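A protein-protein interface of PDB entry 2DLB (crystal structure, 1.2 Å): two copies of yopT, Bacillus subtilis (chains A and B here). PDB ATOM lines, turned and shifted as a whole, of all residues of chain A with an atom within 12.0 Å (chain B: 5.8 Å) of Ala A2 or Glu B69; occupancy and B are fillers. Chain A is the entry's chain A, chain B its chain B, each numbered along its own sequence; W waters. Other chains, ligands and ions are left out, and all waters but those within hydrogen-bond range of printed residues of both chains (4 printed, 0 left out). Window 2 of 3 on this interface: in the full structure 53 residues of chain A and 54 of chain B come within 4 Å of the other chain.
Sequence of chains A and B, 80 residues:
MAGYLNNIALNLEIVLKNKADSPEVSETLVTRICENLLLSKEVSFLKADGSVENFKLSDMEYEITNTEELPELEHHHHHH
The backbone carbonyl oxygen of Ala B20 is in hydrogen-bond range of the backbone NH of Ala A2 (2.8 Å).
The backbone NH (N) of Leu B70 is in hydrogen-bond range of the backbone carbonyl oxygen (O) of Gly A3 (2.7 Å).
O of Asn B18 is in hydrogen-bond range of N of Tyr A4, 3.0 Å away.
O of Leu A5 lies within hydrogen-bond range of N of Glu B68 (2.8 Å).
The side-chain amide oxygen of Asn A6 lies within hydrogen-bond range of the side-chain hydroxyl of Thr B67 (2.7 Å).
Among the printed residues, pairs that only touch across the chains: Ala A2 with Lys B19 (3.2 Å), Tyr A4 with Glu B68 (3.3 Å), Leu A5 with Thr B67 (3.4 Å), Tyr A4 with Ala B20 (3.4 Å), Gly A3 with Asn B18 (3.4 Å), Gly A3 with Glu B69 (3.5 Å), Tyr A4 with Glu B69 (3.6 Å), Ala A2 with Glu B69 (3.7 Å), Tyr A4 with Leu B70 (3.7 Å) and Leu A5 with Leu B70 (3.9 Å).
Glu B69 touches just these residues of chain A: Ala A2 (3.7 Å), Gly A3 (3.5 Å) and Tyr A4 (3.6 Å).
Asn B18 touches just these residues of chain A: Gly A3 and Tyr A4.
Lys B19 touches just one residue of chain A: Ala A2 (3.2 Å).
Ala B20 touches just these residues of chain A: Ala A2 (2.8 Å) and Tyr A4 (3.4 Å).
No residue of chain A comes within 4 Å of Asp B21.
Thr B67 touches just these residues of chain A: Leu A5 and Asn A6.
Glu B68 touches two residues of chain A.
Of chain A, only Gly A3 (2.7 Å), Tyr A4 (3.7 Å) and Leu A5 (3.9 Å) come within 4 Å of Leu B70.
No residue of chain A comes within 4 Å of Pro B71.
Printed residues of chain B within 4 Å of Leu A5: Thr B67 (3.4 Å), Glu B68 (2.8 Å) and Leu B70 (3.9 Å).
Printed residues of chain B within 4 Å of Tyr A4: Asn B18, Ala B20, Glu B68, Glu B69 and Leu B70.
Printed residues of chain B within 4 Å of Gly A3: Asn B18, Glu B69 and Leu B70.
Printed residues of chain B within 4 Å of Asn A6: Thr B67 (2.7 Å).
The nearest residue of chain B that does not touch Ala A2 is Asn B18 (4.1 Å).
Printed residues of chain A that touch a printed residue of chain B: Ala A2, Gly A3, Tyr A4, Leu A5 and Asn A6.
Hydrophobic or aromatic side chains of chain A within 4 Å of the printed part of chain B: Ala A2 and Tyr A4.
Of the 9 printed residues of chain B, 7 touch a printed residue of chain A.
Printed residues of chain B that touch a printed residue of chain A: Asn B18, Lys B19, Ala B20, Thr B67, Glu B68, Glu B69 and Leu B70.
Hydrophobic or aromatic side chains of chain B within 4 Å of the printed part of chain A: Leu B70.
No position is printed for both chains.
Of the 15 pairs that touch across the chains among the printed residues, none has its exchanged pair printed and touching as well.
Water W3 lies within hydrogen-bond range of OH of Tyr A4 (2.7 Å) and OE1 of Glu B69 (2.8 Å).
Water W2 bridges O of Leu B70 and N of Gly A3.
Water W1 lies within hydrogen-bond range of OH of Tyr A4 (2.8 Å) and O of Asp B21 (3.2 Å).
Water W4 lies within hydrogen-bond range of O of Leu A5 (3.0 Å), ND2 of Asn A7 (3.1 Å) and OE2 of Glu B68 (3.3 Å).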
ATOM      1  N   ALA A   2     -17.097  -3.811 -19.352  1.00  0.00           N
ATOM      2  CA  ALA A   2     -16.156  -4.871 -19.695  1.00  0.00           C
ATOM      3  C   ALA A   2     -15.692  -5.453 -18.367  1.00  0.00           C
ATOM      4  O   ALA A   2     -15.829  -4.797 -17.339  1.00  0.00           O
ATOM      5  CB  ALA A   2     -14.973  -4.353 -20.474  1.00  0.00           C
ATOM      6  N   GLY A   3     -15.125  -6.636 -18.465  1.00  0.00           N
ATOM      7  CA  GLY A   3     -14.425  -7.170 -17.313  1.00  0.00           C
ATOM      8  C   GLY A   3     -12.954  -6.783 -17.281  1.00  0.00           C
ATOM      9  O   GLY A   3     -12.308  -6.652 -18.343  1.00  0.00           O
ATOM     10  N   TYR A   4     -12.406  -6.668 -16.066  1.00  0.00           N
ATOM     11  CA  TYR A   4     -11.001  -6.395 -15.867  1.00  0.00           C
ATOM     12  C   TYR A   4     -10.457  -7.273 -14.769  1.00  0.00           C
ATOM     13  O   TYR A   4     -11.118  -7.479 -13.754  1.00  0.00           O
ATOM     14  CB  TYR A   4     -10.714  -4.916 -15.439  1.00  0.00           C
ATOM     15  CG  TYR A   4     -11.126  -3.965 -16.550  1.00  0.00           C
ATOM     16  CD1 TYR A   4     -12.409  -3.470 -16.661  1.00  0.00           C
ATOM     17  CD2 TYR A   4     -10.201  -3.595 -17.529  1.00  0.00           C
ATOM     18  CE1 TYR A   4     -12.729  -2.637 -17.694  1.00  0.00           C
ATOM     19  CE2 TYR A   4     -10.538  -2.760 -18.573  1.00  0.00           C
ATOM     20  CZ  TYR A   4     -11.822  -2.256 -18.643  1.00  0.00           C
ATOM     21  OH  TYR A   4     -12.273  -1.433 -19.636  1.00  0.00           O
ATOM     22  N   LEU A   5      -9.216  -7.698 -14.951  1.00  0.00           N
ATOM     23  CA  LEU A   5      -8.477  -8.390 -13.885  1.00  0.00           C
ATOM     24  C   LEU A   5      -7.440  -7.379 -13.404  1.00  0.00           C
ATOM     25  O   LEU A   5      -6.731  -6.744 -14.241  1.00  0.00           O
ATOM     26  CB  LEU A   5      -7.834  -9.640 -14.447  1.00  0.00           C
ATOM     27  CG  LEU A   5      -7.030 -10.561 -13.578  1.00  0.00           C
ATOM     28  CD1 LEU A   5      -6.957 -11.982 -14.155  1.00  0.00           C
ATOM     29  CD2 LEU A   5      -5.590 -10.073 -13.397  1.00  0.00           C
ATOM     30  N   ASN A   6      -7.286  -7.256 -12.108  1.00  0.00           N
ATOM     31  CA  ASN A   6      -6.246  -6.457 -11.496  1.00  0.00           C
ATOM     32  C   ASN A   6      -5.382  -7.319 -10.586  1.00  0.00           C
ATOM     33  O   ASN A   6      -5.899  -8.155  -9.818  1.00  0.00           O
ATOM     34  CB  ASN A   6      -6.838  -5.351 -10.616  1.00  0.00           C
ATOM     35  CG  ASN A   6      -7.629  -4.324 -11.392  1.00  0.00           C
ATOM     36  OD1 ASN A   6      -7.150  -3.245 -11.736  1.00  0.00           O
ATOM     37  ND2 ASN A   6      -8.876  -4.654 -11.722  1.00  0.00           N
ATOM     38  N   ASN A   7      -4.065  -7.107 -10.680  1.00  0.00           N
ATOM     39  CA  ASN A   7      -3.109  -7.710  -9.754  1.00  0.00           C
ATOM     40  C   ASN A   7      -2.624  -6.598  -8.833  1.00  0.00           C
ATOM     41  O   ASN A   7      -2.240  -5.533  -9.335  1.00  0.00           O
ATOM     42  CB  ASN A   7      -1.930  -8.359 -10.470  1.00  0.00           C
ATOM     43  CG  ASN A   7      -2.416  -9.482 -11.352  1.00  0.00           C
ATOM     44  OD1 ASN A   7      -2.859 -10.539 -10.916  1.00  0.00           O
ATOM     45  ND2 ASN A   7      -2.334  -9.269 -12.627  1.00  0.00           N
ATOM     46  N   ASN B  18     -13.308  -7.250 -11.675  1.00  0.00           N
ATOM     47  CA  ASN B  18     -14.561  -6.510 -11.566  1.00  0.00           C
ATOM     48  C   ASN B  18     -15.035  -6.182 -12.956  1.00  0.00           C
ATOM     49  O   ASN B  18     -14.457  -6.616 -13.943  1.00  0.00           O
ATOM     50  CB  ASN B  18     -14.350  -5.295 -10.664  1.00  0.00           C
ATOM     51  CG  ASN B  18     -13.306  -4.340 -11.190  1.00  0.00           C
ATOM     52  OD1 ASN B  18     -13.125  -4.200 -12.415  1.00  0.00           O
ATOM     53  ND2 ASN B  18     -12.591  -3.683 -10.305  1.00  0.00           N
ATOM     54  N   LYS B  19     -16.140  -5.457 -13.010  1.00  0.00           N
ATOM     55  CA  LYS B  19     -16.748  -5.012 -14.255  1.00  0.00           C
ATOM     56  C   LYS B  19     -16.747  -3.482 -14.228  1.00  0.00           C
ATOM     57  O   LYS B  19     -17.051  -2.882 -13.204  1.00  0.00           O
ATOM     58  CB  LYS B  19     -18.158  -5.552 -14.436  1.00  0.00           C
ATOM     59  CG  LYS B  19     -18.214  -7.087 -14.583  1.00  0.00           C
ATOM     60  CD  LYS B  19     -19.682  -7.490 -14.747  1.00  0.00           C
ATOM     61  CE  LYS B  19     -19.953  -8.916 -15.114  1.00  0.00           C
ATOM     62  NZ  LYS B  19     -21.386  -9.182 -15.472  1.00  0.00           N
ATOM     63  N   ALA B  20     -16.421  -2.796 -15.311  1.00  0.00           N
ATOM     64  CA  ALA B  20     -16.304  -1.369 -15.369  1.00  0.00           C
ATOM     65  C   ALA B  20     -16.293  -0.938 -16.828  1.00  0.00           C
ATOM     66  O   ALA B  20     -16.027  -1.762 -17.718  1.00  0.00           O
ATOM     67  CB  ALA B  20     -15.010  -0.936 -14.703  1.00  0.00           C
ATOM     68  N   ASP B  21     -16.569   0.334 -17.029  1.00  0.00           N
ATOM     69  CA  ASP B  21     -16.580   0.921 -18.348  1.00  0.00           C
ATOM     70  C   ASP B  21     -15.184   1.250 -18.872  1.00  0.00           C
ATOM     71  O   ASP B  21     -15.041   1.653 -20.016  1.00  0.00           O
ATOM     72  CB  ASP B  21     -17.348   2.259 -18.296  1.00  0.00           C
ATOM     73  CG  ASP B  21     -18.785   2.184 -17.896  1.00  0.00           C
ATOM     74  OD1 ASP B  21     -19.356   3.232 -17.474  1.00  0.00           O
ATOM     75  OD2 ASP B  21     -19.367   1.088 -17.997  1.00  0.00           O
ATOM     76  N   THR B  67      -3.607  -3.878 -14.620  1.00  0.00           N
ATOM     77  CA  THR B  67      -5.031  -3.873 -14.882  1.00  0.00           C
ATOM     78  C   THR B  67      -5.191  -4.302 -16.336  1.00  0.00           C
ATOM     79  O   THR B  67      -4.633  -3.645 -17.217  1.00  0.00           O
ATOM     80  CB  THR B  67      -5.657  -2.470 -14.687  1.00  0.00           C
ATOM     81  OG1 THR B  67      -5.359  -2.055 -13.356  1.00  0.00           O
ATOM     82  CG2 THR B  67      -7.163  -2.413 -14.946  1.00  0.00           C
ATOM     83  N   GLU B  68      -5.956  -5.351 -16.551  1.00  0.00           N
ATOM     84  CA  GLU B  68      -6.061  -5.954 -17.829  1.00  0.00           C
ATOM     85  C   GLU B  68      -7.488  -6.264 -18.238  1.00  0.00           C
ATOM     86  O   GLU B  68      -8.202  -6.922 -17.514  1.00  0.00           O
ATOM     87  CB  GLU B  68      -5.133  -7.203 -17.929  1.00  0.00           C
ATOM     88  CG  GLU B  68      -3.647  -6.885 -17.689  1.00  0.00           C
ATOM     89  CD  GLU B  68      -2.722  -8.055 -17.543  1.00  0.00           C
ATOM     90  OE1 GLU B  68      -3.059  -9.189 -17.925  1.00  0.00           O
ATOM     91  OE2 GLU B  68      -1.582  -7.825 -17.023  1.00  0.00           O
ATOM     92  N   GLU B  69      -7.911  -5.816 -19.404  1.00  0.00           N
ATOM     93  CA  GLU B  69      -9.231  -6.120 -19.918  1.00  0.00           C
ATOM     94  C   GLU B  69      -9.398  -7.616 -20.157  1.00  0.00           C
ATOM     95  O   GLU B  69      -8.489  -8.268 -20.681  1.00  0.00           O
ATOM     96  CB  GLU B  69      -9.518  -5.361 -21.212  1.00  0.00           C
ATOM     97  CG  GLU B  69     -10.975  -5.407 -21.612  1.00  0.00           C
ATOM     98  CD  GLU B  69     -11.400  -4.524 -22.761  1.00  0.00           C
ATOM     99  OE1 GLU B  69     -10.586  -3.697 -23.172  1.00  0.00           O
ATOM    100  OE2 GLU B  69     -12.544  -4.642 -23.219  1.00  0.00           O
ATOM    101  N   LEU B  70     -10.526  -8.173 -19.752  1.00  0.00           N
ATOM    102  CA  LEU B  70     -10.804  -9.576 -20.038  1.00  0.00           C
ATOM    103  C   LEU B  70     -11.571  -9.740 -21.312  1.00  0.00           C
ATOM    104  O   LEU B  70     -12.286  -8.892 -21.816  1.00  0.00           O
ATOM    105  CB  LEU B  70     -11.587 -10.132 -18.824  1.00  0.00           C
ATOM    106  CG  LEU B  70     -10.815 -10.161 -17.517  1.00  0.00           C
ATOM    107  CD1 LEU B  70     -11.713 -10.454 -16.304  1.00  0.00           C
ATOM    108  CD2 LEU B  70      -9.708 -11.180 -17.635  1.00  0.00           C
ATOM    109  N   PRO B  71     -11.473 -10.878 -21.993  1.00  0.00           N
ATOM    110  CA  PRO B  71     -12.263 -11.083 -23.212  1.00  0.00           C
ATOM    111  C   PRO B  71     -13.728 -11.306 -22.862  1.00  0.00           C
ATOM    112  O   PRO B  71     -14.575 -10.841 -23.655  1.00  0.00           O
ATOM    113  CB  PRO B  71     -11.631 -12.337 -23.801  1.00  0.00           C
ATOM    114  CG  PRO B  71     -11.022 -13.065 -22.644  1.00  0.00           C
ATOM    115  CD  PRO B  71     -10.627 -12.019 -21.642  1.00  0.00           C
HETATM  116  O   HOH W   1     -14.456  -1.141 -21.426  1.00  0.00           O
HETATM  117  O   HOH W   2     -14.749  -7.946 -20.992  1.00  0.00           O
HETATM  118  O   HOH W   3     -10.664  -1.311 -21.778  1.00  0.00           O
HETATM  119  O   HOH W   4      -4.067  -7.949 -14.821  1.00  0.00           O
